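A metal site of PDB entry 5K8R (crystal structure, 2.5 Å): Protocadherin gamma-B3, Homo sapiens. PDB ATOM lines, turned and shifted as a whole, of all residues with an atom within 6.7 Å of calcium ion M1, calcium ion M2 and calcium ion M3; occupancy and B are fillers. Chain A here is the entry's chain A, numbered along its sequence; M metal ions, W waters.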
ATOM      1  N   GLU A 223       7.576  10.933  22.711  1.00  0.00           N
ATOM      2  CA  GLU A 223       8.969  11.338  22.544  1.00  0.00           C
ATOM      3  C   GLU A 223       9.907  10.501  23.406  1.00  0.00           C
ATOM      4  O   GLU A 223      11.084  10.347  23.062  1.00  0.00           O
ATOM      5  CB  GLU A 223       9.139  12.821  22.865  1.00  0.00           C
ATOM      6  CG  GLU A 223       8.613  13.225  24.224  1.00  0.00           C
ATOM      7  CD  GLU A 223       8.960  14.659  24.579  1.00  0.00           C
ATOM      8  OE1 GLU A 223       9.957  15.176  24.028  1.00  0.00           O
ATOM      9  OE2 GLU A 223       8.234  15.273  25.388  1.00  0.00           O
ATOM     10  N   LEU A 277      13.886  10.444  20.192  1.00  0.00           N
ATOM     11  CA  LEU A 277      12.903  11.420  19.755  1.00  0.00           C
ATOM     12  C   LEU A 277      12.787  12.530  20.785  1.00  0.00           C
ATOM     13  O   LEU A 277      12.805  12.283  21.996  1.00  0.00           O
ATOM     14  CB  LEU A 277      11.547  10.761  19.537  1.00  0.00           C
ATOM     15  CG  LEU A 277      11.377   9.749  18.392  1.00  0.00           C
ATOM     16  CD1 LEU A 277      12.155  10.195  17.160  1.00  0.00           C
ATOM     17  CD2 LEU A 277      11.808   8.353  18.824  1.00  0.00           C
ATOM     18  N   ASP A 278      12.660  13.764  20.304  1.00  0.00           N
ATOM     19  CA  ASP A 278      12.528  14.933  21.173  1.00  0.00           C
ATOM     20  C   ASP A 278      11.427  15.822  20.616  1.00  0.00           C
ATOM     21  O   ASP A 278      11.600  16.446  19.565  1.00  0.00           O
ATOM     22  CB  ASP A 278      13.848  15.692  21.283  1.00  0.00           C
ATOM     23  CG  ASP A 278      13.813  16.769  22.353  1.00  0.00           C
ATOM     24  OD1 ASP A 278      12.943  16.688  23.254  1.00  0.00           O
ATOM     25  OD2 ASP A 278      14.645  17.691  22.302  1.00  0.00           O
ATOM     26  N   PHE A 279      10.292  15.864  21.321  1.00  0.00           N
ATOM     27  CA  PHE A 279       9.174  16.702  20.882  1.00  0.00           C
ATOM     28  C   PHE A 279       9.572  18.175  20.839  1.00  0.00           C
ATOM     29  O   PHE A 279       9.076  18.923  19.986  1.00  0.00           O
ATOM     30  CB  PHE A 279       7.981  16.504  21.810  1.00  0.00           C
ATOM     31  CG  PHE A 279       6.784  17.345  21.462  1.00  0.00           C
ATOM     32  CD1 PHE A 279       5.867  16.909  20.525  1.00  0.00           C
ATOM     33  CD2 PHE A 279       6.582  18.572  22.078  1.00  0.00           C
ATOM     34  CE1 PHE A 279       4.763  17.678  20.207  1.00  0.00           C
ATOM     35  CE2 PHE A 279       5.482  19.350  21.762  1.00  0.00           C
ATOM     36  CZ  PHE A 279       4.568  18.903  20.816  1.00  0.00           C
ATOM     37  N   GLU A 280      10.465  18.604  21.728  1.00  0.00           N
ATOM     38  CA  GLU A 280      10.897  19.993  21.744  1.00  0.00           C
ATOM     39  C   GLU A 280      11.707  20.362  20.516  1.00  0.00           C
ATOM     40  O   GLU A 280      11.793  21.552  20.183  1.00  0.00           O
ATOM     41  CB  GLU A 280      11.707  20.279  23.008  1.00  0.00           C
ATOM     42  CG  GLU A 280      10.870  20.598  24.235  1.00  0.00           C
ATOM     43  CD  GLU A 280       9.999  19.446  24.676  1.00  0.00           C
ATOM     44  OE1 GLU A 280      10.493  18.298  24.696  1.00  0.00           O
ATOM     45  OE2 GLU A 280       8.814  19.681  24.998  1.00  0.00           O
ATOM     46  N   GLU A 281      12.295  19.386  19.825  1.00  0.00           N
ATOM     47  CA  GLU A 281      13.077  19.666  18.628  1.00  0.00           C
ATOM     48  C   GLU A 281      12.249  19.545  17.359  1.00  0.00           C
ATOM     49  O   GLU A 281      12.286  20.429  16.504  1.00  0.00           O
ATOM     50  CB  GLU A 281      14.289  18.732  18.569  1.00  0.00           C
ATOM     51  CG  GLU A 281      15.241  19.024  17.416  1.00  0.00           C
ATOM     52  CD  GLU A 281      15.906  20.386  17.528  1.00  0.00           C
ATOM     53  OE1 GLU A 281      16.103  20.865  18.674  1.00  0.00           O
ATOM     54  OE2 GLU A 281      16.221  20.989  16.488  1.00  0.00           O
ATOM     55  N   SER A 308       4.223  12.968  20.170  1.00  0.00           N
ATOM     56  CA  SER A 308       3.395  13.583  21.187  1.00  0.00           C
ATOM     57  C   SER A 308       4.243  14.068  22.353  1.00  0.00           C
ATOM     58  O   SER A 308       5.308  13.503  22.652  1.00  0.00           O
ATOM     59  CB  SER A 308       2.329  12.600  21.692  1.00  0.00           C
ATOM     60  OG  SER A 308       2.926  11.387  22.119  1.00  0.00           O
ATOM     61  N   ASP A 309       3.766  15.125  23.007  1.00  0.00           N
ATOM     62  CA  ASP A 309       4.546  15.792  24.051  1.00  0.00           C
ATOM     63  C   ASP A 309       4.502  15.006  25.359  1.00  0.00           C
ATOM     64  O   ASP A 309       3.451  14.486  25.751  1.00  0.00           O
ATOM     65  CB  ASP A 309       4.022  17.212  24.267  1.00  0.00           C
ATOM     66  CG  ASP A 309       4.815  17.963  25.320  1.00  0.00           C
ATOM     67  OD1 ASP A 309       6.039  17.754  25.412  1.00  0.00           O
ATOM     68  OD2 ASP A 309       4.201  18.773  26.058  1.00  0.00           O
ATOM     69  N   GLU A 310       5.657  14.928  26.020  1.00  0.00           N
ATOM     70  CA  GLU A 310       5.769  14.336  27.340  1.00  0.00           C
ATOM     71  C   GLU A 310       6.376  15.360  28.296  1.00  0.00           C
ATOM     72  O   GLU A 310       7.141  16.239  27.890  1.00  0.00           O
ATOM     73  CB  GLU A 310       6.648  13.074  27.323  1.00  0.00           C
ATOM     74  CG  GLU A 310       5.952  11.850  26.748  1.00  0.00           C
ATOM     75  CD  GLU A 310       5.004  11.205  27.737  1.00  0.00           C
ATOM     76  OE1 GLU A 310       5.427  10.948  28.883  1.00  0.00           O
ATOM     77  OE2 GLU A 310       3.835  10.960  27.382  1.00  0.00           O
ATOM     78  N   ASN A 311       6.012  15.241  29.571  1.00  0.00           N
ATOM     79  CA  ASN A 311       6.463  16.201  30.587  1.00  0.00           C
ATOM     80  C   ASN A 311       7.834  15.776  31.114  1.00  0.00           C
ATOM     81  O   ASN A 311       7.991  15.272  32.226  1.00  0.00           O
ATOM     82  CB  ASN A 311       5.439  16.298  31.712  1.00  0.00           C
ATOM     83  CG  ASN A 311       5.723  17.456  32.648  1.00  0.00           C
ATOM     84  OD1 ASN A 311       6.381  18.431  32.277  1.00  0.00           O
ATOM     85  ND2 ASN A 311       5.215  17.362  33.870  1.00  0.00           N
ATOM     86  N   ASP A 312       8.848  15.987  30.266  1.00  0.00           N
ATOM     87  CA  ASP A 312      10.220  15.625  30.589  1.00  0.00           C
ATOM     88  C   ASP A 312      11.134  16.829  30.739  1.00  0.00           C
ATOM     89  O   ASP A 312      12.350  16.715  30.615  1.00  0.00           O
ATOM     90  CB  ASP A 312      10.782  14.672  29.528  1.00  0.00           C
ATOM     91  CG  ASP A 312      10.917  15.333  28.162  1.00  0.00           C
ATOM     92  OD1 ASP A 312      10.136  16.263  27.864  1.00  0.00           O
ATOM     93  OD2 ASP A 312      11.804  14.915  27.395  1.00  0.00           O
ATOM     94  N   ASN A 313      10.561  18.010  31.010  1.00  0.00           N
ATOM     95  CA  ASN A 313      11.327  19.222  31.241  1.00  0.00           C
ATOM     96  C   ASN A 313      10.777  19.926  32.469  1.00  0.00           C
ATOM     97  O   ASN A 313       9.600  20.283  32.502  1.00  0.00           O
ATOM     98  CB  ASN A 313      11.270  20.153  30.019  1.00  0.00           C
ATOM     99  CG  ASN A 313      12.148  19.670  28.873  1.00  0.00           C
ATOM    100  OD1 ASN A 313      13.315  20.058  28.775  1.00  0.00           O
ATOM    101  ND2 ASN A 313      11.585  18.838  28.018  1.00  0.00           N
ATOM    102  N   ALA A 314      11.635  20.117  33.466  1.00  0.00           N
ATOM    103  CA  ALA A 314      11.232  20.763  34.702  1.00  0.00           C
ATOM    104  C   ALA A 314      11.154  22.275  34.530  1.00  0.00           C
ATOM    105  O   ALA A 314      11.888  22.851  33.714  1.00  0.00           O
ATOM    106  CB  ALA A 314      12.203  20.426  35.831  1.00  0.00           C
ATOM    107  N   PRO A 315      10.259  22.947  35.256  1.00  0.00           N
ATOM    108  CA  PRO A 315      10.179  24.412  35.160  1.00  0.00           C
ATOM    109  C   PRO A 315      11.472  25.065  35.621  1.00  0.00           C
ATOM    110  O   PRO A 315      12.187  24.538  36.482  1.00  0.00           O
ATOM    111  CB  PRO A 315       9.010  24.768  36.090  1.00  0.00           C
ATOM    112  CG  PRO A 315       8.213  23.504  36.195  1.00  0.00           C
ATOM    113  CD  PRO A 315       9.207  22.398  36.119  1.00  0.00           C
ATOM    114  N   ASP A 343       9.089  27.007  30.865  1.00  0.00           N
ATOM    115  CA  ASP A 343       9.055  25.558  30.731  1.00  0.00           C
ATOM    116  C   ASP A 343       9.073  25.208  29.252  1.00  0.00           C
ATOM    117  O   ASP A 343       8.300  25.765  28.469  1.00  0.00           O
ATOM    118  CB  ASP A 343       7.821  24.965  31.408  1.00  0.00           C
ATOM    119  CG  ASP A 343       7.937  23.469  31.653  1.00  0.00           C
ATOM    120  OD1 ASP A 343       7.688  23.023  32.793  1.00  0.00           O
ATOM    121  OD2 ASP A 343       8.294  22.733  30.705  1.00  0.00           O
ATOM    122  N   LEU A 344       9.952  24.283  28.873  1.00  0.00           N
ATOM    123  CA  LEU A 344      10.126  23.944  27.466  1.00  0.00           C
ATOM    124  C   LEU A 344       9.000  23.089  26.907  1.00  0.00           C
ATOM    125  O   LEU A 344       8.853  22.998  25.681  1.00  0.00           O
ATOM    126  CB  LEU A 344      11.461  23.224  27.261  1.00  0.00           C
ATOM    127  CG  LEU A 344      12.724  23.983  27.662  1.00  0.00           C
ATOM    128  CD1 LEU A 344      13.966  23.132  27.437  1.00  0.00           C
ATOM    129  CD2 LEU A 344      12.835  25.304  26.905  1.00  0.00           C
ATOM    130  N   ASP A 345       8.197  22.467  27.765  1.00  0.00           N
ATOM    131  CA  ASP A 345       7.135  21.580  27.311  1.00  0.00           C
ATOM    132  C   ASP A 345       5.936  22.397  26.816  1.00  0.00           C
ATOM    133  O   ASP A 345       5.908  23.623  26.906  1.00  0.00           O
ATOM    134  CB  ASP A 345       6.733  20.613  28.421  1.00  0.00           C
ATOM    135  CG  ASP A 345       7.866  19.713  28.845  1.00  0.00           C
ATOM    136  OD1 ASP A 345       8.716  19.378  27.988  1.00  0.00           O
ATOM    137  OD2 ASP A 345       7.925  19.332  30.036  1.00  0.00           O
ATOM    138  N   SER A 346       4.935  21.701  26.288  1.00  0.00           N
ATOM    139  CA  SER A 346       3.754  22.331  25.720  1.00  0.00           C
ATOM    140  C   SER A 346       2.515  21.939  26.518  1.00  0.00           C
ATOM    141  O   SER A 346       2.532  20.999  27.309  1.00  0.00           O
ATOM    142  CB  SER A 346       3.579  21.929  24.251  1.00  0.00           C
ATOM    143  OG  SER A 346       4.739  22.208  23.497  1.00  0.00           O
ATOM    144  N   PHE A 348      -0.465  21.848  29.225  1.00  0.00           N
ATOM    145  CA  PHE A 348      -0.406  21.918  30.675  1.00  0.00           C
ATOM    146  C   PHE A 348       0.940  21.443  31.216  1.00  0.00           C
ATOM    147  O   PHE A 348       1.283  21.773  32.358  1.00  0.00           O
ATOM    148  CB  PHE A 348      -1.538  21.099  31.295  1.00  0.00           C
ATOM    149  CG  PHE A 348      -2.870  21.813  31.285  1.00  0.00           C
ATOM    150  CD1 PHE A 348      -3.120  22.859  32.149  1.00  0.00           C
ATOM    151  CD2 PHE A 348      -3.867  21.427  30.402  1.00  0.00           C
ATOM    152  CE1 PHE A 348      -4.336  23.519  32.146  1.00  0.00           C
ATOM    153  CE2 PHE A 348      -5.086  22.083  30.383  1.00  0.00           C
ATOM    154  CZ  PHE A 348      -5.321  23.127  31.262  1.00  0.00           C
ATOM    155  N   ASN A 349       1.705  20.685  30.427  1.00  0.00           N
ATOM    156  CA  ASN A 349       3.065  20.368  30.814  1.00  0.00           C
ATOM    157  C   ASN A 349       3.950  21.608  30.862  1.00  0.00           C
ATOM    158  O   ASN A 349       4.993  21.592  31.519  1.00  0.00           O
ATOM    159  CB  ASN A 349       3.669  19.341  29.845  1.00  0.00           C
ATOM    160  CG  ASN A 349       2.828  18.091  29.717  1.00  0.00           C
ATOM    161  OD1 ASN A 349       2.206  17.632  30.682  1.00  0.00           O
ATOM    162  ND2 ASN A 349       2.787  17.523  28.511  1.00  0.00           N
ATOM    163  N   GLY A 350       3.540  22.681  30.179  1.00  0.00           N
ATOM    164  CA  GLY A 350       4.309  23.908  30.165  1.00  0.00           C
ATOM    165  C   GLY A 350       3.731  25.000  31.036  1.00  0.00           C
ATOM    166  O   GLY A 350       4.406  26.001  31.305  1.00  0.00           O
ATOM    167  N   GLU A 351       2.492  24.833  31.492  1.00  0.00           N
ATOM    168  CA  GLU A 351       1.908  25.779  32.425  1.00  0.00           C
ATOM    169  C   GLU A 351       2.631  25.702  33.758  1.00  0.00           C
ATOM    170  O   GLU A 351       2.993  24.617  34.221  1.00  0.00           O
ATOM    171  CB  GLU A 351       0.411  25.494  32.612  1.00  0.00           C
ATOM    172  CG  GLU A 351      -0.400  25.533  31.329  1.00  0.00           C
ATOM    173  CD  GLU A 351      -0.474  26.920  30.718  1.00  0.00           C
ATOM    174  OE1 GLU A 351      -0.316  27.912  31.460  1.00  0.00           O
ATOM    175  OE2 GLU A 351      -0.690  27.020  29.490  1.00  0.00           O
ATOM    176  N   ASP A 396       5.055  22.583  37.373  1.00  0.00           N
ATOM    177  CA  ASP A 396       4.208  22.551  36.193  1.00  0.00           C
ATOM    178  C   ASP A 396       2.928  21.776  36.477  1.00  0.00           C
ATOM    179  O   ASP A 396       2.730  21.235  37.572  1.00  0.00           O
ATOM    180  CB  ASP A 396       4.968  21.969  34.998  1.00  0.00           C
ATOM    181  CG  ASP A 396       5.571  20.605  35.295  1.00  0.00           C
ATOM    182  OD1 ASP A 396       5.059  19.880  36.164  1.00  0.00           O
ATOM    183  OD2 ASP A 396       6.580  20.250  34.642  1.00  0.00           O
ATOM    184  N   LYS A 397       2.043  21.716  35.486  1.00  0.00           N
ATOM    185  CA  LYS A 397       0.761  21.039  35.614  1.00  0.00           C
ATOM    186  C   LYS A 397       0.697  19.766  34.777  1.00  0.00           C
ATOM    187  O   LYS A 397      -0.361  19.388  34.275  1.00  0.00           O
ATOM    188  CB  LYS A 397      -0.379  21.982  35.217  1.00  0.00           C
ATOM    189  CG  LYS A 397      -0.343  23.327  35.947  1.00  0.00           C
ATOM    190  CD  LYS A 397      -1.558  24.162  35.611  1.00  0.00           C
ATOM    191  CE  LYS A 397      -1.421  25.575  36.174  1.00  0.00           C
ATOM    192  NZ  LYS A 397      -1.168  25.571  37.638  1.00  0.00           N
ATOM    193  N   GLY A 398       1.837  19.074  34.634  1.00  0.00           N
ATOM    194  CA  GLY A 398       1.888  17.842  33.883  1.00  0.00           C
ATOM    195  C   GLY A 398       1.575  16.624  34.737  1.00  0.00           C
ATOM    196  O   GLY A 398       1.322  16.716  35.938  1.00  0.00           O
ATOM    197  N   LEU A 402       6.339  18.133  37.493  1.00  0.00           N
ATOM    198  CA  LEU A 402       7.733  18.387  37.806  1.00  0.00           C
ATOM    199  C   LEU A 402       7.876  19.770  38.421  1.00  0.00           C
ATOM    200  O   LEU A 402       7.054  20.658  38.175  1.00  0.00           O
ATOM    201  CB  LEU A 402       8.636  18.276  36.560  1.00  0.00           C
ATOM    202  CG  LEU A 402       9.080  16.871  36.130  1.00  0.00           C
ATOM    203  CD1 LEU A 402       7.921  16.066  35.546  1.00  0.00           C
ATOM    204  CD2 LEU A 402      10.216  16.957  35.130  1.00  0.00           C
HETATM  205 CA    CA M   1       7.244  20.721  32.057  1.00  0.00          CA
HETATM  206 CA    CA M   2       8.368  17.573  26.250  1.00  0.00          CA
HETATM  207 CA    CA M   3      11.687  16.301  25.391  1.00  0.00          CA
HETATM  208  O   HOH W   1      14.210  17.105  27.649  1.00  0.00           O
HETATM  209  O   HOH W   2      13.497  14.701  24.647  1.00  0.00           O
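ND2 of Asn 313 sits close to OD1 of Asp 312, 3.0 Å away.
The backbone NH of Phe 279 lies close to the side-chain carboxylate of Glu 223 (2.8 Å).
The backbone NH (N) of Glu 223 sits at hydrogen-bond distance from the backbone carbonyl oxygen (O) of Ser 308 (3.4 Å).
The side-chain amide nitrogen (ND2) of Asn 349 lies within hydrogen-bond range of the side-chain carboxylate (OD2) of Asp 309 (3.1 Å).
The side-chain carboxylate (OD2) of Asp 309 is in hydrogen-bond range of the backbone NH (N) of Ser 346 (3.0 Å).
The side-chain carboxylate (OD1) of Asp 396 is in hydrogen-bond range of the backbone NH (N) of Leu 402 (2.5 Å).
Six residues have an atom within 4 Å of calcium ion M1: Asn 311, Asn 313, Asp 343, Asp 345, Asn 349 and Asp 396.
The nearest printed residue that does not touch calcium ion M1 is Gly 350 (4.6 Å).
Seven residues have an atom within 4 Å of calcium ion M2: Glu 223, Glu 280, Asp 309, Glu 310, Asp 312, Asn 313 and Asp 345.
The nearest printed residue that does not touch calcium ion M3 is Phe 279 (4.3 Å).
Calcium ion M1 is bound by the backbone carbonyl oxygen (O) of Asn 313, the side-chain carboxylate (OD1) of Asp 343, the side-chain amide oxygen (OD1) of Asn 311, the backbone carbonyl oxygen (O) of Asn 349, the side-chain carboxylate (OD2) of Asp 345, the side-chain carboxylate (OD2) of Asp 343 and the side-chain carboxylate (OD2) of Asp 396.
Calcium ion M2 is bound by the backbone carbonyl oxygen (O) of Glu 310 (2.4 Å), the side-chain carboxylate (OE2) of Glu 223 (2.5 Å), the side-chain carboxylate (OD1) of Asp 309 (2.5 Å), the side-chain carboxylate (OE2) of Glu 280 (2.5 Å), the side-chain carboxylate (OD1) of Asp 345 (2.5 Å), the side-chain carboxylate (OD1) of Asp 312 (2.7 Å) and the side-chain carboxylate (OE1) of Glu 280 (2.7 Å).
Calcium ion M2 has seven donor atoms within binding distance.
Calcium ion M3 is bound by the side-chain carboxylate of Glu 280, the side-chain carboxylate of Asp 312, the side-chain carboxylate of Glu 223, the side-chain carboxylate of Asp 278 and water W2.
Slightly farther from calcium ion M3 lies OD1 of Asp 312 (2.9 Å).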
